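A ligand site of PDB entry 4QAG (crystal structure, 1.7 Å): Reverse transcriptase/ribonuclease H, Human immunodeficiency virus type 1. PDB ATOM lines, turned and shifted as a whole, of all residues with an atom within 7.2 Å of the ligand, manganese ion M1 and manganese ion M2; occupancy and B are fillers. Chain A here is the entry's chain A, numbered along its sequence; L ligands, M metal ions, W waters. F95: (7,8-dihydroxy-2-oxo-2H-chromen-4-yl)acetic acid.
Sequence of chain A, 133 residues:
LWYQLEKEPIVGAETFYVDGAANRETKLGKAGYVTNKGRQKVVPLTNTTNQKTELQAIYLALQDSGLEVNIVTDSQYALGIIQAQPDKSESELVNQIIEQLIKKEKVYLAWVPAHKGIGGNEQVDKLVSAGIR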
ATOM      1  N   VAL A  18     -23.232  24.840 -12.829  1.00  0.00           N
ATOM      2  CA  VAL A  18     -22.054  25.467 -12.258  1.00  0.00           C
ATOM      3  C   VAL A  18     -21.875  25.095 -10.791  1.00  0.00           C
ATOM      4  O   VAL A  18     -22.851  24.866 -10.077  1.00  0.00           O
ATOM      5  CB  VAL A  18     -22.100  27.017 -12.403  1.00  0.00           C
ATOM      6  CG1 VAL A  18     -22.143  27.432 -13.869  1.00  0.00           C
ATOM      7  CG2 VAL A  18     -23.278  27.594 -11.664  1.00  0.00           C
ATOM      8  N   ASP A  19     -20.633  25.062 -10.317  1.00  0.00           N
ATOM      9  CA  ASP A  19     -20.387  24.884  -8.881  1.00  0.00           C
ATOM     10  C   ASP A  19     -18.994  25.349  -8.564  1.00  0.00           C
ATOM     11  O   ASP A  19     -18.142  25.484  -9.452  1.00  0.00           O
ATOM     12  CB  ASP A  19     -20.578  23.423  -8.456  1.00  0.00           C
ATOM     13  CG  ASP A  19     -20.832  23.255  -6.954  1.00  0.00           C
ATOM     14  OD1 ASP A  19     -20.615  22.159  -6.410  1.00  0.00           O
ATOM     15  OD2 ASP A  19     -21.247  24.244  -6.316  1.00  0.00           O
ATOM     16  N   GLY A  20     -18.738  25.548  -7.287  1.00  0.00           N
ATOM     17  CA  GLY A  20     -17.423  25.911  -6.817  1.00  0.00           C
ATOM     18  C   GLY A  20     -17.196  25.198  -5.507  1.00  0.00           C
ATOM     19  O   GLY A  20     -18.156  24.767  -4.845  1.00  0.00           O
ATOM     20  N   ALA A  21     -15.925  25.051  -5.141  1.00  0.00           N
ATOM     21  CA  ALA A  21     -15.588  24.482  -3.840  1.00  0.00           C
ATOM     22  C   ALA A  21     -14.329  25.183  -3.346  1.00  0.00           C
ATOM     23  O   ALA A  21     -13.438  25.475  -4.139  1.00  0.00           O
ATOM     24  CB  ALA A  21     -15.351  22.998  -3.961  1.00  0.00           C
ATOM     25  N   ASN A  50     -15.733  30.150  -0.637  1.00  0.00           N
ATOM     26  CA  ASN A  50     -16.811  29.425  -1.296  1.00  0.00           C
ATOM     27  C   ASN A  50     -17.631  30.323  -2.220  1.00  0.00           C
ATOM     28  O   ASN A  50     -17.863  29.986  -3.382  1.00  0.00           O
ATOM     29  CB  ASN A  50     -17.738  28.758  -0.267  1.00  0.00           C
ATOM     30  CG  ASN A  50     -17.153  27.479   0.305  1.00  0.00           C
ATOM     31  OD1 ASN A  50     -17.043  27.326   1.527  1.00  0.00           O
ATOM     32  ND2 ASN A  50     -16.765  26.560  -0.569  1.00  0.00           N
ATOM     33  N   GLN A  51     -18.086  31.464  -1.705  1.00  0.00           N
ATOM     34  CA  GLN A  51     -18.961  32.324  -2.496  1.00  0.00           C
ATOM     35  C   GLN A  51     -18.265  32.883  -3.722  1.00  0.00           C
ATOM     36  O   GLN A  51     -18.888  33.030  -4.781  1.00  0.00           O
ATOM     37  CB  GLN A  51     -19.537  33.463  -1.651  1.00  0.00           C
ATOM     38  CG  GLN A  51     -20.669  33.020  -0.725  1.00  0.00           C
ATOM     39  CD  GLN A  51     -20.167  32.507   0.606  1.00  0.00           C
ATOM     40  OE1 GLN A  51     -18.953  32.372   0.819  1.00  0.00           O
ATOM     41  NE2 GLN A  51     -21.088  32.228   1.524  1.00  0.00           N
ATOM     42  N   THR A  53     -15.927  31.335  -5.394  1.00  0.00           N
ATOM     43  CA  THR A  53     -15.829  30.255  -6.383  1.00  0.00           C
ATOM     44  C   THR A  53     -17.157  30.062  -7.080  1.00  0.00           C
ATOM     45  O   THR A  53     -17.206  29.765  -8.256  1.00  0.00           O
ATOM     46  CB  THR A  53     -15.358  28.887  -5.781  1.00  0.00           C
ATOM     47  OG1 THR A  53     -16.346  28.383  -4.872  1.00  0.00           O
ATOM     48  CG2 THR A  53     -14.010  29.016  -5.074  1.00  0.00           C
ATOM     49  N   GLU A  54     -18.264  30.260  -6.371  1.00  0.00           N
ATOM     50  CA  GLU A  54     -19.560  30.055  -6.991  1.00  0.00           C
ATOM     51  C   GLU A  54     -19.811  31.147  -8.032  1.00  0.00           C
ATOM     52  O   GLU A  54     -20.424  30.890  -9.070  1.00  0.00           O
ATOM     53  CB  GLU A  54     -20.676  30.044  -5.937  1.00  0.00           C
ATOM     54  CG  GLU A  54     -20.545  28.913  -4.915  1.00  0.00           C
ATOM     55  CD  GLU A  54     -21.250  27.630  -5.320  1.00  0.00           C
ATOM     56  OE1 GLU A  54     -21.782  27.549  -6.452  1.00  0.00           O
ATOM     57  OE2 GLU A  54     -21.285  26.689  -4.490  1.00  0.00           O
ATOM     58  N   THR A  73     -27.463  26.895 -10.767  1.00  0.00           N
ATOM     59  CA  THR A  73     -26.542  27.042  -9.638  1.00  0.00           C
ATOM     60  C   THR A  73     -27.178  26.475  -8.372  1.00  0.00           C
ATOM     61  O   THR A  73     -28.388  26.371  -8.282  1.00  0.00           O
ATOM     62  CB  THR A  73     -26.215  28.528  -9.366  1.00  0.00           C
ATOM     63  OG1 THR A  73     -25.293  28.637  -8.271  1.00  0.00           O
ATOM     64  CG2 THR A  73     -27.468  29.309  -9.024  1.00  0.00           C
ATOM     65  N   ASP A  74     -26.348  26.121  -7.391  1.00  0.00           N
ATOM     66  CA  ASP A  74     -26.865  25.708  -6.089  1.00  0.00           C
ATOM     67  C   ASP A  74     -26.610  26.800  -5.044  1.00  0.00           C
ATOM     68  O   ASP A  74     -26.817  26.588  -3.848  1.00  0.00           O
ATOM     69  CB  ASP A  74     -26.249  24.351  -5.645  1.00  0.00           C
ATOM     70  CG  ASP A  74     -24.739  24.448  -5.340  1.00  0.00           C
ATOM     71  OD1 ASP A  74     -24.275  25.530  -5.000  1.00  0.00           O
ATOM     72  OD2 ASP A  74     -23.993  23.441  -5.424  1.00  0.00           O
ATOM     73  N   SER A  75     -26.113  27.954  -5.504  1.00  0.00           N
ATOM     74  CA  SER A  75     -25.737  29.061  -4.625  1.00  0.00           C
ATOM     75  C   SER A  75     -26.825  30.140  -4.538  1.00  0.00           C
ATOM     76  O   SER A  75     -27.010  30.912  -5.463  1.00  0.00           O
ATOM     77  CB  SER A  75     -24.439  29.711  -5.108  1.00  0.00           C
ATOM     78  OG  SER A  75     -24.110  30.883  -4.364  1.00  0.00           O
ATOM     79  N   GLN A  76     -27.519  30.198  -3.406  1.00  0.00           N
ATOM     80  CA  GLN A  76     -28.459  31.287  -3.145  1.00  0.00           C
ATOM     81  C   GLN A  76     -27.806  32.670  -3.114  1.00  0.00           C
ATOM     82  O   GLN A  76     -28.413  33.678  -3.500  1.00  0.00           O
ATOM     83  CB  GLN A  76     -29.195  31.022  -1.826  1.00  0.00           C
ATOM     84  CG  GLN A  76     -30.259  29.941  -1.935  1.00  0.00           C
ATOM     85  CD  GLN A  76     -31.629  30.477  -2.300  1.00  0.00           C
ATOM     86  OE1 GLN A  76     -32.060  31.509  -1.784  1.00  0.00           O
ATOM     87  NE2 GLN A  76     -32.319  29.794  -3.191  1.00  0.00           N
ATOM     88  N   TYR A  77     -26.556  32.719  -2.653  1.00  0.00           N
ATOM     89  CA  TYR A  77     -25.762  33.945  -2.597  1.00  0.00           C
ATOM     90  C   TYR A  77     -25.642  34.578  -3.987  1.00  0.00           C
ATOM     91  O   TYR A  77     -25.926  35.752  -4.176  1.00  0.00           O
ATOM     92  CB  TYR A  77     -24.378  33.577  -2.049  1.00  0.00           C
ATOM     93  CG  TYR A  77     -23.449  34.739  -1.730  1.00  0.00           C
ATOM     94  CD1 TYR A  77     -23.423  35.321  -0.458  1.00  0.00           C
ATOM     95  CD2 TYR A  77     -22.572  35.236  -2.685  1.00  0.00           C
ATOM     96  CE1 TYR A  77     -22.556  36.356  -0.171  1.00  0.00           C
ATOM     97  CE2 TYR A  77     -21.715  36.274  -2.408  1.00  0.00           C
ATOM     98  CZ  TYR A  77     -21.704  36.839  -1.138  1.00  0.00           C
ATOM     99  OH  TYR A  77     -20.850  37.874  -0.848  1.00  0.00           O
ATOM    100  N   ALA A  78     -25.172  33.793  -4.958  1.00  0.00           N
ATOM    101  CA  ALA A  78     -25.071  34.288  -6.324  1.00  0.00           C
ATOM    102  C   ALA A  78     -26.435  34.630  -6.911  1.00  0.00           C
ATOM    103  O   ALA A  78     -26.573  35.644  -7.599  1.00  0.00           O
ATOM    104  CB  ALA A  78     -24.368  33.239  -7.202  1.00  0.00           C
ATOM    105  N   TRP A 111     -32.004  27.922  -9.634  1.00  0.00           N
ATOM    106  CA  TRP A 111     -31.398  27.392  -8.420  1.00  0.00           C
ATOM    107  C   TRP A 111     -31.915  25.990  -8.114  1.00  0.00           C
ATOM    108  O   TRP A 111     -33.118  25.695  -8.276  1.00  0.00           O
ATOM    109  CB  TRP A 111     -31.729  28.295  -7.233  1.00  0.00           C
ATOM    110  CG  TRP A 111     -31.158  27.788  -5.947  1.00  0.00           C
ATOM    111  CD1 TRP A 111     -29.884  27.952  -5.492  1.00  0.00           C
ATOM    112  CD2 TRP A 111     -31.844  26.998  -4.960  1.00  0.00           C
ATOM    113  NE1 TRP A 111     -29.737  27.322  -4.270  1.00  0.00           N
ATOM    114  CE2 TRP A 111     -30.919  26.723  -3.934  1.00  0.00           C
ATOM    115  CE3 TRP A 111     -33.146  26.494  -4.851  1.00  0.00           C
ATOM    116  CZ2 TRP A 111     -31.260  25.991  -2.797  1.00  0.00           C
ATOM    117  CZ3 TRP A 111     -33.477  25.762  -3.734  1.00  0.00           C
ATOM    118  CH2 TRP A 111     -32.541  25.503  -2.723  1.00  0.00           C
ATOM    119  N   PRO A 113     -31.170  22.790  -4.942  1.00  0.00           N
ATOM    120  CA  PRO A 113     -30.489  22.544  -3.678  1.00  0.00           C
ATOM    121  C   PRO A 113     -29.296  21.623  -3.887  1.00  0.00           C
ATOM    122  O   PRO A 113     -29.383  20.658  -4.626  1.00  0.00           O
ATOM    123  CB  PRO A 113     -31.542  21.814  -2.831  1.00  0.00           C
ATOM    124  CG  PRO A 113     -32.816  21.855  -3.635  1.00  0.00           C
ATOM    125  CD  PRO A 113     -32.425  22.033  -5.044  1.00  0.00           C
ATOM    126  N   ALA A 114     -28.193  21.921  -3.210  1.00  0.00           N
ATOM    127  CA  ALA A 114     -26.992  21.115  -3.337  1.00  0.00           C
ATOM    128  C   ALA A 114     -27.195  19.722  -2.735  1.00  0.00           C
ATOM    129  O   ALA A 114     -27.888  19.559  -1.727  1.00  0.00           O
ATOM    130  CB  ALA A 114     -25.816  21.832  -2.665  1.00  0.00           C
ATOM    131  N   HIS A 115     -26.590  18.725  -3.369  1.00  0.00           N
ATOM    132  CA  HIS A 115     -26.573  17.353  -2.883  1.00  0.00           C
ATOM    133  C   HIS A 115     -27.977  16.804  -2.689  1.00  0.00           C
ATOM    134  O   HIS A 115     -28.287  16.208  -1.650  1.00  0.00           O
ATOM    135  CB  HIS A 115     -25.785  17.269  -1.569  1.00  0.00           C
ATOM    136  CG  HIS A 115     -24.386  17.793  -1.695  1.00  0.00           C
ATOM    137  ND1 HIS A 115     -23.419  17.180  -2.474  1.00  0.00           N
ATOM    138  CD2 HIS A 115     -23.786  18.873  -1.143  1.00  0.00           C
ATOM    139  CE1 HIS A 115     -22.299  17.865  -2.397  1.00  0.00           C
ATOM    140  NE2 HIS A 115     -22.490  18.895  -1.598  1.00  0.00           N
ATOM    141  N   ASN A 121     -25.976  19.005 -11.515  1.00  0.00           N
ATOM    142  CA  ASN A 121     -25.430  19.606 -10.308  1.00  0.00           C
ATOM    143  C   ASN A 121     -24.478  18.664  -9.577  1.00  0.00           C
ATOM    144  O   ASN A 121     -23.399  19.077  -9.144  1.00  0.00           O
ATOM    145  CB  ASN A 121     -26.559  20.046  -9.377  1.00  0.00           C
ATOM    146  CG  ASN A 121     -26.063  20.512  -8.032  1.00  0.00           C
ATOM    147  OD1 ASN A 121     -26.078  19.762  -7.057  1.00  0.00           O
ATOM    148  ND2 ASN A 121     -25.609  21.753  -7.966  1.00  0.00           N
ATOM    149  N   GLU A 122     -24.869  17.411  -9.426  1.00  0.00           N
ATOM    150  CA  GLU A 122     -24.018  16.452  -8.724  1.00  0.00           C
ATOM    151  C   GLU A 122     -22.726  16.241  -9.515  1.00  0.00           C
ATOM    152  O   GLU A 122     -21.641  16.112  -8.942  1.00  0.00           O
ATOM    153  CB  GLU A 122     -24.753  15.131  -8.504  1.00  0.00           C
ATOM    154  CG  GLU A 122     -25.954  15.225  -7.555  1.00  0.00           C
ATOM    155  CD  GLU A 122     -25.561  15.300  -6.077  1.00  0.00           C
ATOM    156  OE1 GLU A 122     -24.477  15.850  -5.766  1.00  0.00           O
ATOM    157  OE2 GLU A 122     -26.338  14.824  -5.223  1.00  0.00           O
ATOM    158  N   VAL A 124     -21.013  18.336 -11.542  1.00  0.00           N
ATOM    159  CA  VAL A 124     -20.066  19.425 -11.407  1.00  0.00           C
ATOM    160  C   VAL A 124     -19.545  19.532  -9.971  1.00  0.00           C
ATOM    161  O   VAL A 124     -18.383  19.856  -9.760  1.00  0.00           O
ATOM    162  CB  VAL A 124     -20.636  20.773 -11.908  1.00  0.00           C
ATOM    163  CG1 VAL A 124     -21.847  21.206 -11.082  1.00  0.00           C
ATOM    164  CG2 VAL A 124     -19.558  21.829 -11.902  1.00  0.00           C
ATOM    165  N   ASP A 125     -20.404  19.254  -9.003  1.00  0.00           N
ATOM    166  CA  ASP A 125     -19.955  19.221  -7.614  1.00  0.00           C
ATOM    167  C   ASP A 125     -18.751  18.300  -7.458  1.00  0.00           C
ATOM    168  O   ASP A 125     -17.728  18.700  -6.893  1.00  0.00           O
ATOM    169  CB  ASP A 125     -21.075  18.783  -6.667  1.00  0.00           C
ATOM    170  CG  ASP A 125     -20.568  18.533  -5.245  1.00  0.00           C
ATOM    171  OD1 ASP A 125     -20.323  19.513  -4.512  1.00  0.00           O
ATOM    172  OD2 ASP A 125     -20.402  17.346  -4.874  1.00  0.00           O
ATOM    173  N   LYS A 126     -18.866  17.082  -7.970  1.00  0.00           N
ATOM    174  CA  LYS A 126     -17.781  16.110  -7.866  1.00  0.00           C
ATOM    175  C   LYS A 126     -16.512  16.616  -8.531  1.00  0.00           C
ATOM    176  O   LYS A 126     -15.406  16.390  -8.040  1.00  0.00           O
ATOM    177  CB  LYS A 126     -18.200  14.769  -8.457  1.00  0.00           C
ATOM    178  CG  LYS A 126     -19.267  14.042  -7.636  1.00  0.00           C
ATOM    179  CD  LYS A 126     -19.538  12.628  -8.161  1.00  0.00           C
ATOM    180  CE  LYS A 126     -20.488  11.857  -7.246  1.00  0.00           C
ATOM    181  NZ  LYS A 126     -21.851  12.461  -7.189  1.00  0.00           N
ATOM    182  N   VAL A 128     -15.469  19.944  -9.062  1.00  0.00           N
ATOM    183  CA  VAL A 128     -14.813  21.039  -8.357  1.00  0.00           C
ATOM    184  C   VAL A 128     -14.419  20.661  -6.938  1.00  0.00           C
ATOM    185  O   VAL A 128     -13.568  21.325  -6.331  1.00  0.00           O
ATOM    186  CB  VAL A 128     -15.677  22.309  -8.314  1.00  0.00           C
ATOM    187  CG1 VAL A 128     -16.041  22.754  -9.720  1.00  0.00           C
ATOM    188  CG2 VAL A 128     -16.927  22.091  -7.461  1.00  0.00           C
ATOM    189  N   SER A 129     -15.022  19.617  -6.388  1.00  0.00           N
ATOM    190  CA  SER A 129     -14.772  19.270  -4.992  1.00  0.00           C
ATOM    191  C   SER A 129     -13.540  18.367  -4.836  1.00  0.00           C
ATOM    192  O   SER A 129     -12.864  18.397  -3.811  1.00  0.00           O
ATOM    193  CB  SER A 129     -16.017  18.624  -4.366  1.00  0.00           C
ATOM    194  OG  SER A 129     -15.722  17.352  -3.824  1.00  0.00           O
HETATM  195  C1  F95 L   1     -23.321  23.942  -0.375  1.00  0.00           C
HETATM  196  C2  F95 L   1     -22.816  24.130  -1.668  1.00  0.00           C
HETATM  197  C3  F95 L   1     -22.067  23.120  -2.274  1.00  0.00           C
HETATM  198  C4  F95 L   1     -21.845  21.924  -1.595  1.00  0.00           C
HETATM  199  C5  F95 L   1     -22.343  21.708  -0.309  1.00  0.00           C
HETATM  200  C6  F95 L   1     -23.088  22.719   0.315  1.00  0.00           C
HETATM  201  O1  F95 L   1     -21.568  23.268  -3.534  1.00  0.00           O
HETATM  202  O2  F95 L   1     -21.119  20.955  -2.175  1.00  0.00           O
HETATM  203  O3  F95 L   1     -23.052  25.322  -2.314  1.00  0.00           O
HETATM  204  C7  F95 L   1     -23.765  26.390  -1.825  1.00  0.00           C
HETATM  205  C8  F95 L   1     -24.315  26.164  -0.419  1.00  0.00           C
HETATM  206  C9  F95 L   1     -24.098  25.009   0.246  1.00  0.00           C
HETATM  207  O4  F95 L   1     -23.950  27.435  -2.427  1.00  0.00           O
HETATM  208  C10 F95 L   1     -24.639  24.764   1.657  1.00  0.00           C
HETATM  209  C11 F95 L   1     -25.587  23.560   1.789  1.00  0.00           C
HETATM  210  O5  F95 L   1     -26.501  23.443   0.947  1.00  0.00           O
HETATM  211  O6  F95 L   1     -25.346  22.762   2.733  1.00  0.00           O
HETATM  212 MN    MN M   1     -20.922  21.558  -4.310  1.00  0.00          MN
HETATM  213 MN    MN M   2     -22.333  24.907  -4.653  1.00  0.00          MN
HETATM  214  O   HOH W   1     -27.041  28.218  -1.236  1.00  0.00           O
HETATM  215  O   HOH W   2     -23.714  22.782   4.638  1.00  0.00           O
HETATM  216  O   HOH W   3     -18.850  22.162  -3.828  1.00  0.00           O
HETATM  217  O   HOH W   4     -23.004  21.071  -4.754  1.00  0.00           O
HETATM  218  O   HOH W   5     -22.592  29.845  -2.025  1.00  0.00           O
HETATM  219  O   HOH W   6     -27.725  24.676  -2.050  1.00  0.00           O
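Manganese ion M2 is bound by OD1 of Asp 74 (2.1 Å), OE2 of Glu 54 (2.1 Å), OD2 of Asp 19 (2.1 Å), O1 of the ligand (2.1 Å), OD2 of Asp 74 (2.3 Å) and O3 of the ligand (2.5 Å).
Manganese ion M1 is bound by an oxygen (O1) of the ligand (2.0 Å), the side-chain carboxylate (OD1) of Asp 125 (2.1 Å), water W4 (2.2 Å), the side-chain carboxylate (OD1) of Asp 19 (2.2 Å), water W3 (2.2 Å) and an oxygen (O2) of the ligand (2.2 Å).
The side-chain carboxylate (OD2) of Asp 74 lies close to the side-chain amide nitrogen (ND2) of Asn 121 (3.5 Å). The backbone carbonyl oxygen (O) of Asp 74 is in hydrogen-bond range of the indole nitrogen (NE1) of Trp 111. The side-chain hydroxyl of Thr 73 is in hydrogen-bond range of the backbone NH of Ser 75. N of Ala 78 lies within hydrogen-bond range of OG of Ser 75, 3.2 Å away.
Of the 25 residues printed, 3 come within 4 Å of manganese ion M1.
Three residues have an atom within 4 Å of manganese ion M2: Asp 19, Glu 54 and Asp 74. The nearest printed residue that does not touch manganese ion M2 is Gly 20 (4.2 Å).
O of Gly 20 touches O1 of the ligand (3.95 Å). Ser 75 touches the ligand. CB of Ala 114 touches C2 of the ligand, at 3.9 Å. Hydrophobic or aromatic side chains that line the ligand: Ala 114 and His 115. Within 4 Å of the ligand: Asp 19, Gly 20, Glu 54, Asp 74, Ser 75, Ala 114, His 115 and Asp 125.
An oxygen (O2) of the ligand lies close to a ring nitrogen (NE2) of His 115 (2.5 Å).
Water W5 lies within hydrogen-bond range of an oxygen (O4) of the ligand (2.8 Å) and the side-chain hydroxyl (OG) of Ser 75 (3.0 Å). Water W1 lies within hydrogen-bond range of N of Gln 76 (3.0 Å), O of Asp 74 (3.1 Å) and O4 of the ligand (3.4 Å). Water W6 lies within hydrogen-bond range of O of Asp 74 (2.8 Å), N of Ala 114 (3.0 Å) and O5 of the ligand (3.5 Å).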
